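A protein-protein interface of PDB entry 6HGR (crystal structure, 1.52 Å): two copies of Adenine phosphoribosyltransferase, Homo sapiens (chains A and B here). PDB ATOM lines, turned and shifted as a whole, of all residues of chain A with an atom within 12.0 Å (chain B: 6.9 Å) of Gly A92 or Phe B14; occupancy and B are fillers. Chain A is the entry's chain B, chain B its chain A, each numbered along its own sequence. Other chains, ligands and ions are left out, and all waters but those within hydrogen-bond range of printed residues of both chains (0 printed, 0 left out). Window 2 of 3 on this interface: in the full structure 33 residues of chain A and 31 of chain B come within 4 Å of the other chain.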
ATOM      1  N   LEU A  83       2.428  10.861   3.171  1.00  0.00           N
ATOM      2  CA  LEU A  83       3.007   9.538   3.182  1.00  0.00           C
ATOM      3  C   LEU A  83       2.333   8.642   4.210  1.00  0.00           C
ATOM      4  O   LEU A  83       2.151   9.037   5.381  1.00  0.00           O
ATOM      5  CB  LEU A  83       4.482   9.621   3.555  1.00  0.00           C
ATOM      6  CG  LEU A  83       5.335  10.553   2.699  1.00  0.00           C
ATOM      7  CD1 LEU A  83       6.783  10.545   3.176  1.00  0.00           C
ATOM      8  CD2 LEU A  83       5.228  10.134   1.248  1.00  0.00           C
ATOM      9  N   ARG A  85       3.325   5.118   5.873  1.00  0.00           N
ATOM     10  CA  ARG A  85       4.548   4.336   5.964  1.00  0.00           C
ATOM     11  C   ARG A  85       4.337   3.044   6.713  1.00  0.00           C
ATOM     12  O   ARG A  85       3.397   2.911   7.489  1.00  0.00           O
ATOM     13  CB  ARG A  85       5.623   5.135   6.693  1.00  0.00           C
ATOM     14  CG  ARG A  85       6.045   6.405   5.980  1.00  0.00           C
ATOM     15  CD  ARG A  85       7.556   6.498   5.933  1.00  0.00           C
ATOM     16  NE  ARG A  85       8.120   5.254   5.420  1.00  0.00           N
ATOM     17  CZ  ARG A  85       9.416   4.958   5.408  1.00  0.00           C
ATOM     18  NH1 ARG A  85      10.303   5.811   5.897  1.00  0.00           N
ATOM     19  NH2 ARG A  85       9.821   3.795   4.909  1.00  0.00           N
ATOM     20  N   LYS A  86       5.213   2.075   6.480  1.00  0.00           N
ATOM     21  CA  LYS A  86       5.295   0.929   7.373  1.00  0.00           C
ATOM     22  C   LYS A  86       5.568   1.416   8.797  1.00  0.00           C
ATOM     23  O   LYS A  86       6.330   2.361   9.006  1.00  0.00           O
ATOM     24  CB  LYS A  86       6.395  -0.018   6.896  1.00  0.00           C
ATOM     25  CG  LYS A  86       6.110  -0.615   5.526  1.00  0.00           C
ATOM     26  CD  LYS A  86       4.913  -1.547   5.575  1.00  0.00           C
ATOM     27  CE  LYS A  86       5.226  -2.816   6.351  1.00  0.00           C
ATOM     28  NZ  LYS A  86       6.135  -3.721   5.593  1.00  0.00           N
ATOM     29  N   ARG A  87       4.920   0.790   9.777  1.00  0.00           N
ATOM     30  CA  ARG A  87       5.043   1.230  11.158  1.00  0.00           C
ATOM     31  C   ARG A  87       6.483   1.232  11.661  1.00  0.00           C
ATOM     32  O   ARG A  87       7.264   0.338  11.333  1.00  0.00           O
ATOM     33  CB  ARG A  87       4.184   0.371  12.086  1.00  0.00           C
ATOM     34  CG  ARG A  87       4.246   0.839  13.529  1.00  0.00           C
ATOM     35  CD  ARG A  87       3.262   0.117  14.426  1.00  0.00           C
ATOM     36  NE  ARG A  87       3.393   0.573  15.804  1.00  0.00           N
ATOM     37  CZ  ARG A  87       2.912  -0.084  16.855  1.00  0.00           C
ATOM     38  NH1 ARG A  87       3.071   0.392  18.082  1.00  0.00           N
ATOM     39  NH2 ARG A  87       2.274  -1.228  16.671  1.00  0.00           N
ATOM     40  N   GLY A  88       6.817   2.261  12.441  1.00  0.00           N
ATOM     41  CA  GLY A  88       8.118   2.350  13.107  1.00  0.00           C
ATOM     42  C   GLY A  88       9.074   3.382  12.542  1.00  0.00           C
ATOM     43  O   GLY A  88      10.167   3.580  13.081  1.00  0.00           O
ATOM     44  N   LYS A  89       8.677   4.052  11.467  1.00  0.00           N
ATOM     45  CA  LYS A  89       9.606   4.896  10.721  1.00  0.00           C
ATOM     46  C   LYS A  89       9.355   6.396  10.910  1.00  0.00           C
ATOM     47  O   LYS A  89      10.215   7.226  10.599  1.00  0.00           O
ATOM     48  CB  LYS A  89       9.522   4.547   9.238  1.00  0.00           C
ATOM     49  CG  LYS A  89       9.859   3.097   8.926  1.00  0.00           C
ATOM     50  CD  LYS A  89      11.342   2.827   9.117  1.00  0.00           C
ATOM     51  CE  LYS A  89      11.699   1.391   8.773  1.00  0.00           C
ATOM     52  NZ  LYS A  89      13.137   1.104   9.034  1.00  0.00           N
ATOM     53  N   LEU A  90       8.169   6.741  11.395  1.00  0.00           N
ATOM     54  CA  LEU A  90       7.743   8.126  11.475  1.00  0.00           C
ATOM     55  C   LEU A  90       7.955   8.721  12.874  1.00  0.00           C
ATOM     56  O   LEU A  90       7.601   8.120  13.894  1.00  0.00           O
ATOM     57  CB  LEU A  90       6.269   8.242  11.059  1.00  0.00           C
ATOM     58  CG  LEU A  90       5.992   7.992   9.573  1.00  0.00           C
ATOM     59  CD1 LEU A  90       4.512   7.786   9.315  1.00  0.00           C
ATOM     60  CD2 LEU A  90       6.515   9.152   8.741  1.00  0.00           C
ATOM     61  N   PRO A  91       8.536   9.931  12.935  1.00  0.00           N
ATOM     62  CA  PRO A  91       8.639  10.648  14.189  1.00  0.00           C
ATOM     63  C   PRO A  91       7.326  11.354  14.483  1.00  0.00           C
ATOM     64  O   PRO A  91       6.491  11.496  13.585  1.00  0.00           O
ATOM     65  CB  PRO A  91       9.727  11.682  13.883  1.00  0.00           C
ATOM     66  CG  PRO A  91       9.483  12.013  12.460  1.00  0.00           C
ATOM     67  CD  PRO A  91       9.046  10.728  11.806  1.00  0.00           C
ATOM     68  N   GLY A  92       7.150  11.786  15.722  1.00  0.00           N
ATOM     69  CA  GLY A  92       5.939  12.491  16.134  1.00  0.00           C
ATOM     70  C   GLY A  92       4.816  11.522  16.448  1.00  0.00           C
ATOM     71  O   GLY A  92       4.952  10.316  16.280  1.00  0.00           O
ATOM     72  N   PRO A  93       3.696  12.057  16.904  1.00  0.00           N
ATOM     73  CA  PRO A  93       2.561  11.210  17.257  1.00  0.00           C
ATOM     74  C   PRO A  93       1.973  10.562  16.014  1.00  0.00           C
ATOM     75  O   PRO A  93       1.869  11.217  14.968  1.00  0.00           O
ATOM     76  CB  PRO A  93       1.569  12.196  17.868  1.00  0.00           C
ATOM     77  CG  PRO A  93       2.412  13.325  18.357  1.00  0.00           C
ATOM     78  CD  PRO A  93       3.520  13.442  17.356  1.00  0.00           C
ATOM     79  N   THR A  94       1.615   9.289  16.129  1.00  0.00           N
ATOM     80  CA  THR A  94       1.141   8.531  14.990  1.00  0.00           C
ATOM     81  C   THR A  94      -0.054   7.676  15.337  1.00  0.00           C
ATOM     82  O   THR A  94      -0.396   7.495  16.514  1.00  0.00           O
ATOM     83  CB  THR A  94       2.206   7.587  14.406  1.00  0.00           C
ATOM     84  OG1 THR A  94       2.534   6.585  15.366  1.00  0.00           O
ATOM     85  CG2 THR A  94       3.457   8.344  13.980  1.00  0.00           C
ATOM     86  N   LEU A  95      -0.730   7.257  14.273  1.00  0.00           N
ATOM     87  CA  LEU A  95      -1.799   6.268  14.284  1.00  0.00           C
ATOM     88  C   LEU A  95      -1.356   5.113  13.412  1.00  0.00           C
ATOM     89  O   LEU A  95      -0.678   5.327  12.403  1.00  0.00           O
ATOM     90  CB  LEU A  95      -3.062   6.834  13.632  1.00  0.00           C
ATOM     91  CG  LEU A  95      -3.749   8.066  14.189  1.00  0.00           C
ATOM     92  CD1 LEU A  95      -5.086   8.222  13.477  1.00  0.00           C
ATOM     93  CD2 LEU A  95      -3.935   7.922  15.691  1.00  0.00           C
ATOM     94  N   TRP A  96      -1.761   3.894  13.731  1.00  0.00           N
ATOM     95  CA  TRP A  96      -1.366   2.761  12.901  1.00  0.00           C
ATOM     96  C   TRP A  96      -2.514   1.775  12.742  1.00  0.00           C
ATOM     97  O   TRP A  96      -3.498   1.814  13.480  1.00  0.00           O
ATOM     98  CB  TRP A  96      -0.122   2.063  13.464  1.00  0.00           C
ATOM     99  CG  TRP A  96      -0.308   1.496  14.826  1.00  0.00           C
ATOM    100  CD1 TRP A  96      -0.880   0.305  15.150  1.00  0.00           C
ATOM    101  CD2 TRP A  96       0.081   2.105  16.058  1.00  0.00           C
ATOM    102  NE1 TRP A  96      -0.870   0.135  16.509  1.00  0.00           N
ATOM    103  CE2 TRP A  96      -0.294   1.234  17.088  1.00  0.00           C
ATOM    104  CE3 TRP A  96       0.710   3.303  16.385  1.00  0.00           C
ATOM    105  CZ2 TRP A  96      -0.055   1.524  18.426  1.00  0.00           C
ATOM    106  CZ3 TRP A  96       0.938   3.591  17.703  1.00  0.00           C
ATOM    107  CH2 TRP A  96       0.567   2.706  18.709  1.00  0.00           C
ATOM    108  N   LEU A 108       0.616  -0.315   8.885  1.00  0.00           N
ATOM    109  CA  LEU A 108       0.877   0.969   8.265  1.00  0.00           C
ATOM    110  C   LEU A 108       0.653   2.065   9.293  1.00  0.00           C
ATOM    111  O   LEU A 108      -0.071   1.865  10.281  1.00  0.00           O
ATOM    112  CB  LEU A 108      -0.067   1.202   7.084  1.00  0.00           C
ATOM    113  CG  LEU A 108       0.100   0.334   5.835  1.00  0.00           C
ATOM    114  CD1 LEU A 108      -0.932   0.755   4.804  1.00  0.00           C
ATOM    115  CD2 LEU A 108       1.506   0.474   5.301  1.00  0.00           C
ATOM    116  N   GLU A 109       1.275   3.213   9.071  1.00  0.00           N
ATOM    117  CA  GLU A 109       1.268   4.294  10.064  1.00  0.00           C
ATOM    118  C   GLU A 109       1.221   5.656   9.374  1.00  0.00           C
ATOM    119  O   GLU A 109       1.704   5.808   8.257  1.00  0.00           O
ATOM    120  CB  GLU A 109       2.534   4.163  10.926  1.00  0.00           C
ATOM    121  CG  GLU A 109       2.693   5.116  12.091  1.00  0.00           C
ATOM    122  CD  GLU A 109       3.887   4.737  12.977  1.00  0.00           C
ATOM    123  OE1 GLU A 109       3.735   4.691  14.223  1.00  0.00           O
ATOM    124  OE2 GLU A 109       4.970   4.466  12.426  1.00  0.00           O
ATOM    125  N   ILE A 110       0.602   6.634  10.021  1.00  0.00           N
ATOM    126  CA  ILE A 110       0.544   8.000   9.513  1.00  0.00           C
ATOM    127  C   ILE A 110       0.720   8.967  10.678  1.00  0.00           C
ATOM    128  O   ILE A 110       0.315   8.656  11.788  1.00  0.00           O
ATOM    129  CB  ILE A 110      -0.787   8.277   8.769  1.00  0.00           C
ATOM    130  CG1 ILE A 110      -0.709   9.569   7.960  1.00  0.00           C
ATOM    131  CG2 ILE A 110      -1.946   8.337   9.739  1.00  0.00           C
ATOM    132  CD1 ILE A 110      -1.854   9.721   6.971  1.00  0.00           C
ATOM    133  N   GLN A 111       1.363  10.107  10.444  1.00  0.00           N
ATOM    134  CA  GLN A 111       1.464  11.141  11.471  1.00  0.00           C
ATOM    135  C   GLN A 111       0.071  11.718  11.756  1.00  0.00           C
ATOM    136  O   GLN A 111      -0.721  11.914  10.837  1.00  0.00           O
ATOM    137  CB  GLN A 111       2.463  12.229  11.027  1.00  0.00           C
ATOM    138  CG  GLN A 111       3.905  11.720  10.976  1.00  0.00           C
ATOM    139  CD  GLN A 111       4.907  12.716  10.384  1.00  0.00           C
ATOM    140  OE1 GLN A 111       4.629  13.398   9.400  1.00  0.00           O
ATOM    141  NE2 GLN A 111       6.084  12.791  10.984  1.00  0.00           N
ATOM    142  N   LYS A 112      -0.254  11.905  13.034  1.00  0.00           N
ATOM    143  CA  LYS A 112      -1.561  12.450  13.419  1.00  0.00           C
ATOM    144  C   LYS A 112      -1.781  13.833  12.805  1.00  0.00           C
ATOM    145  O   LYS A 112      -2.919  14.235  12.629  1.00  0.00           O
ATOM    146  CB  LYS A 112      -1.736  12.540  14.940  1.00  0.00           C
ATOM    147  CG  LYS A 112      -1.711  11.228  15.700  1.00  0.00           C
ATOM    148  CD  LYS A 112      -2.250  11.441  17.116  1.00  0.00           C
ATOM    149  CE  LYS A 112      -1.916  10.281  18.038  1.00  0.00           C
ATOM    150  NZ  LYS A 112      -2.435  10.460  19.422  1.00  0.00           N
ATOM    151  N   ASP A 113      -0.698  14.523  12.431  1.00  0.00           N
ATOM    152  CA  ASP A 113      -0.815  15.851  11.819  1.00  0.00           C
ATOM    153  C   ASP A 113      -0.700  15.847  10.289  1.00  0.00           C
ATOM    154  O   ASP A 113      -0.518  16.898   9.666  1.00  0.00           O
ATOM    155  CB  ASP A 113       0.172  16.850  12.460  1.00  0.00           C
ATOM    156  CG  ASP A 113       1.624  16.595  12.065  1.00  0.00           C
ATOM    157  OD1 ASP A 113       1.894  15.630  11.329  1.00  0.00           O
ATOM    158  OD2 ASP A 113       2.499  17.385  12.483  1.00  0.00           O
ATOM    159  N   ALA A 114      -0.852  14.685   9.653  1.00  0.00           N
ATOM    160  CA  ALA A 114      -0.652  14.633   8.205  1.00  0.00           C
ATOM    161  C   ALA A 114      -1.742  15.399   7.447  1.00  0.00           C
ATOM    162  O   ALA A 114      -1.491  16.004   6.403  1.00  0.00           O
ATOM    163  CB  ALA A 114      -0.570  13.199   7.719  1.00  0.00           C
ATOM    164  N   LEU A 144      -8.232  10.219  10.726  1.00  0.00           N
ATOM    165  CA  LEU A 144      -7.870  11.645  10.723  1.00  0.00           C
ATOM    166  C   LEU A 144      -9.035  12.518  10.290  1.00  0.00           C
ATOM    167  O   LEU A 144      -8.901  13.732  10.189  1.00  0.00           O
ATOM    168  CB  LEU A 144      -6.684  11.910   9.800  1.00  0.00           C
ATOM    169  CG  LEU A 144      -5.363  11.263  10.199  1.00  0.00           C
ATOM    170  CD1 LEU A 144      -4.265  11.657   9.219  1.00  0.00           C
ATOM    171  CD2 LEU A 144      -5.011  11.635  11.628  1.00  0.00           C
ATOM    172  N   ARG B  12      11.782  19.323   9.067  1.00  0.00           N
ATOM    173  CA  ARG B  12      11.342  19.375  10.445  1.00  0.00           C
ATOM    174  C   ARG B  12      12.281  18.479  11.266  1.00  0.00           C
ATOM    175  O   ARG B  12      12.576  17.356  10.867  1.00  0.00           O
ATOM    176  CB  ARG B  12       9.908  18.837  10.467  1.00  0.00           C
ATOM    177  CG  ARG B  12       9.170  18.910  11.768  1.00  0.00           C
ATOM    178  CD  ARG B  12       7.684  18.828  11.481  1.00  0.00           C
ATOM    179  NE  ARG B  12       7.306  17.572  10.850  1.00  0.00           N
ATOM    180  CZ  ARG B  12       6.057  17.128  10.801  1.00  0.00           C
ATOM    181  NH1 ARG B  12       5.091  17.847  11.351  1.00  0.00           N
ATOM    182  NH2 ARG B  12       5.779  15.974  10.208  1.00  0.00           N
ATOM    183  N   SER B  13      12.798  19.001  12.371  1.00  0.00           N
ATOM    184  CA  SER B  13      13.789  18.283  13.166  1.00  0.00           C
ATOM    185  C   SER B  13      13.216  17.855  14.505  1.00  0.00           C
ATOM    186  O   SER B  13      12.678  18.690  15.241  1.00  0.00           O
ATOM    187  CB  SER B  13      15.014  19.175  13.378  1.00  0.00           C
ATOM    188  OG  SER B  13      15.615  19.480  12.124  1.00  0.00           O
ATOM    189  N   PHE B  14      13.262  16.550  14.779  1.00  0.00           N
ATOM    190  CA  PHE B  14      12.705  15.950  15.997  1.00  0.00           C
ATOM    191  C   PHE B  14      13.829  15.459  16.889  1.00  0.00           C
ATOM    192  O   PHE B  14      14.577  14.560  16.493  1.00  0.00           O
ATOM    193  CB  PHE B  14      11.830  14.731  15.651  1.00  0.00           C
ATOM    194  CG  PHE B  14      10.507  15.077  15.011  1.00  0.00           C
ATOM    195  CD1 PHE B  14      10.416  15.261  13.645  1.00  0.00           C
ATOM    196  CD2 PHE B  14       9.361  15.200  15.781  1.00  0.00           C
ATOM    197  CE1 PHE B  14       9.208  15.580  13.042  1.00  0.00           C
ATOM    198  CE2 PHE B  14       8.147  15.529  15.186  1.00  0.00           C
ATOM    199  CZ  PHE B  14       8.067  15.682  13.814  1.00  0.00           C
ATOM    200  N   PRO B  15      13.965  16.021  18.088  1.00  0.00           N
ATOM    201  CA  PRO B  15      14.994  15.544  19.004  1.00  0.00           C
ATOM    202  C   PRO B  15      14.633  14.198  19.585  1.00  0.00           C
ATOM    203  O   PRO B  15      13.455  13.888  19.755  1.00  0.00           O
ATOM    204  CB  PRO B  15      15.003  16.602  20.101  1.00  0.00           C
ATOM    205  CG  PRO B  15      13.597  17.130  20.105  1.00  0.00           C
ATOM    206  CD  PRO B  15      13.166  17.111  18.677  1.00  0.00           C
ATOM    207  N   ASP B  16      15.648  13.410  19.918  1.00  0.00           N
ATOM    208  CA  ASP B  16      15.473  12.149  20.649  1.00  0.00           C
ATOM    209  C   ASP B  16      14.663  11.096  19.913  1.00  0.00           C
ATOM    210  O   ASP B  16      13.985  10.287  20.544  1.00  0.00           O
ATOM    211  CB  ASP B  16      14.911  12.397  22.048  1.00  0.00           C
ATOM    212  CG  ASP B  16      15.713  13.428  22.805  1.00  0.00           C
ATOM    213  OD1 ASP B  16      16.960  13.306  22.863  1.00  0.00           O
ATOM    214  OD2 ASP B  16      15.108  14.386  23.334  1.00  0.00           O
ATOM    215  N   PHE B  17      14.795  11.071  18.592  1.00  0.00           N
ATOM    216  CA  PHE B  17      14.170  10.046  17.753  1.00  0.00           C
ATOM    217  C   PHE B  17      15.181   9.523  16.742  1.00  0.00           C
ATOM    218  O   PHE B  17      15.785  10.317  16.030  1.00  0.00           O
ATOM    219  CB  PHE B  17      12.977  10.620  16.976  1.00  0.00           C
ATOM    220  CG  PHE B  17      12.225   9.579  16.193  1.00  0.00           C
ATOM    221  CD1 PHE B  17      11.257   8.803  16.817  1.00  0.00           C
ATOM    222  CD2 PHE B  17      12.520   9.336  14.862  1.00  0.00           C
ATOM    223  CE1 PHE B  17      10.585   7.819  16.116  1.00  0.00           C
ATOM    224  CE2 PHE B  17      11.854   8.347  14.158  1.00  0.00           C
ATOM    225  CZ  PHE B  17      10.883   7.591  14.789  1.00  0.00           C
ATOM    226  N   PRO B  18      15.377   8.202  16.669  1.00  0.00           N
ATOM    227  CA  PRO B  18      14.633   7.226  17.457  1.00  0.00           C
ATOM    228  C   PRO B  18      15.196   6.947  18.854  1.00  0.00           C
ATOM    229  O   PRO B  18      14.577   6.220  19.620  1.00  0.00           O
ATOM    230  CB  PRO B  18      14.721   5.960  16.606  1.00  0.00           C
ATOM    231  CG  PRO B  18      16.008   6.094  15.865  1.00  0.00           C
ATOM    232  CD  PRO B  18      16.184   7.567  15.614  1.00  0.00           C
ATOM    233  N   VAL B  22      19.828  11.966  19.525  1.00  0.00           N
ATOM    234  CA  VAL B  22      19.896  12.099  18.078  1.00  0.00           C
ATOM    235  C   VAL B  22      18.732  12.932  17.581  1.00  0.00           C
ATOM    236  O   VAL B  22      17.649  12.925  18.172  1.00  0.00           O
ATOM    237  CB  VAL B  22      19.870  10.725  17.402  1.00  0.00           C
ATOM    238  CG1 VAL B  22      20.911   9.817  18.044  1.00  0.00           C
ATOM    239  CG2 VAL B  22      18.493  10.101  17.490  1.00  0.00           C
ATOM    240  N   VAL B  23      18.979  13.689  16.527  1.00  0.00           N
ATOM    241  CA  VAL B  23      17.961  14.555  15.988  1.00  0.00           C
ATOM    242  C   VAL B  23      17.558  13.997  14.635  1.00  0.00           C
ATOM    243  O   VAL B  23      18.383  13.875  13.742  1.00  0.00           O
ATOM    244  CB  VAL B  23      18.468  16.005  15.869  1.00  0.00           C
ATOM    245  CG1 VAL B  23      17.415  16.887  15.230  1.00  0.00           C
ATOM    246  CG2 VAL B  23      18.850  16.536  17.242  1.00  0.00           C
ATOM    247  N   PHE B  24      16.277  13.669  14.482  1.00  0.00           N
ATOM    248  CA  PHE B  24      15.782  13.077  13.252  1.00  0.00           C
ATOM    249  C   PHE B  24      15.363  14.187  12.310  1.00  0.00           C
ATOM    250  O   PHE B  24      14.579  15.050  12.674  1.00  0.00           O
ATOM    251  CB  PHE B  24      14.584  12.173  13.571  1.00  0.00           C
ATOM    252  CG  PHE B  24      14.045  11.435  12.388  1.00  0.00           C
ATOM    253  CD1 PHE B  24      13.112  12.018  11.552  1.00  0.00           C
ATOM    254  CD2 PHE B  24      14.464  10.145  12.125  1.00  0.00           C
ATOM    255  CE1 PHE B  24      12.605  11.326  10.456  1.00  0.00           C
ATOM    256  CE2 PHE B  24      13.955   9.445  11.048  1.00  0.00           C
ATOM    257  CZ  PHE B  24      13.030  10.038  10.213  1.00  0.00           C
ATOM    258  N   ARG B  25      15.879  14.190  11.086  1.00  0.00           N
ATOM    259  CA  ARG B  25      15.448  15.180  10.105  1.00  0.00           C
ATOM    260  C   ARG B  25      14.336  14.626   9.237  1.00  0.00           C
ATOM    261  O   ARG B  25      14.532  13.663   8.509  1.00  0.00           O
ATOM    262  CB  ARG B  25      16.620  15.598   9.220  1.00  0.00           C
ATOM    263  CG  ARG B  25      17.878  15.924   9.991  1.00  0.00           C
ATOM    264  CD  ARG B  25      17.721  17.151  10.865  1.00  0.00           C
ATOM    265  NE  ARG B  25      18.902  17.318  11.703  1.00  0.00           N
ATOM    266  CZ  ARG B  25      19.176  18.391  12.429  1.00  0.00           C
ATOM    267  NH1 ARG B  25      18.366  19.429  12.452  1.00  0.00           N
ATOM    268  NH2 ARG B  25      20.289  18.415  13.148  1.00  0.00           N
ATOM    269  N   ASP B  26      13.156  15.226   9.352  1.00  0.00           N
ATOM    270  CA  ASP B  26      11.950  14.729   8.684  1.00  0.00           C
ATOM    271  C   ASP B  26      11.744  15.526   7.404  1.00  0.00           C
ATOM    272  O   ASP B  26      11.510  16.734   7.451  1.00  0.00           O
ATOM    273  CB  ASP B  26      10.761  14.897   9.634  1.00  0.00           C
ATOM    274  CG  ASP B  26       9.434  14.441   9.032  1.00  0.00           C
ATOM    275  OD1 ASP B  26       9.443  13.665   8.053  1.00  0.00           O
ATOM    276  OD2 ASP B  26       8.386  14.840   9.595  1.00  0.00           O
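Among the printed residues, pairs that only touch across the chains: Leu A90 with Phe B17 (3.4 Å), Pro A91 with Phe B14 (3.6 Å), Pro A91 with Phe B24 (3.7 Å), Pro A91 with Phe B17 (3.8 Å), Gly A92 with Phe B14 (3.9 Å) and Lys A89 with Phe B24 (3.998 Å).
Of the printed residues of chain A, Phe B14 touches Pro A91 and Gly A92.
Arg B12 touches just these residues of chain A: Gln A111 (2.9 Å) and Asp A113 (2.9 Å).
No residue of chain A comes within 4 Å of Asp B16.
Of the printed residues of chain B, Asp A113 touches Arg B12.
Of the printed residues of chain B, Lys A89 touches Phe B24 (3.998 Å).
Printed residues of chain A within 4 Å of Phe B24: Lys A89 and Pro A91.
Of the printed residues of chain B, Pro A91 touches Phe B14, Phe B17 and Phe B24.
Lys A86 touches none of the printed residues of chain B.
Leu A83 touches none of the printed residues of chain B.
The nearest residue of chain B that does not touch Gly A92 is Phe B17 (5.2 Å).
The nearest printed residue of chain B that does not touch Gln A111 is Phe B14 (4.5 Å).
The guanidinium group (NH2) of Arg B12 is in salt-bridge range of the side-chain carboxylate (OD2) of Asp B26 (2.9 Å).
The backbone NH (N) of Phe B24 sits at hydrogen-bond distance from the backbone carbonyl oxygen (O) of Phe B14, at 2.8 Å.
O of Val B22 is in hydrogen-bond range of N of Phe B17, 3.4 Å away.
O of Pro A91 sits at hydrogen-bond distance from NE2 of Gln A111 (2.9 Å).
Printed residues of chain B that touch a printed residue of chain A: Arg B12, Phe B14, Phe B17, Phe B24 and Asp B26.
Hydrophobic or aromatic side chains of chain B that line the printed part of chain A: Phe B14, Phe B17 and Phe B24.
Along chain B the printed residues that touch a printed residue of chain A span positions 12 to 26.
Among the printed residues, 9 pairs touch across the chains.
No position is printed for both chains.
Of the 9 pairs that touch across the chains among the printed residues, none has its exchanged pair printed and touching as well.
The guanidinium group (NH2) of Arg B12 sits at hydrogen-bond distance from the side-chain amide oxygen (OE1) of Gln A111 (2.9 Å).
The guanidinium group (NH1) of Arg B12 is in salt-bridge range of the side-chain carboxylate (OD2) of Asp A113.
OD2 of Asp B26 is in hydrogen-bond range of NE2 of Gln A111, at 3.4 Å.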
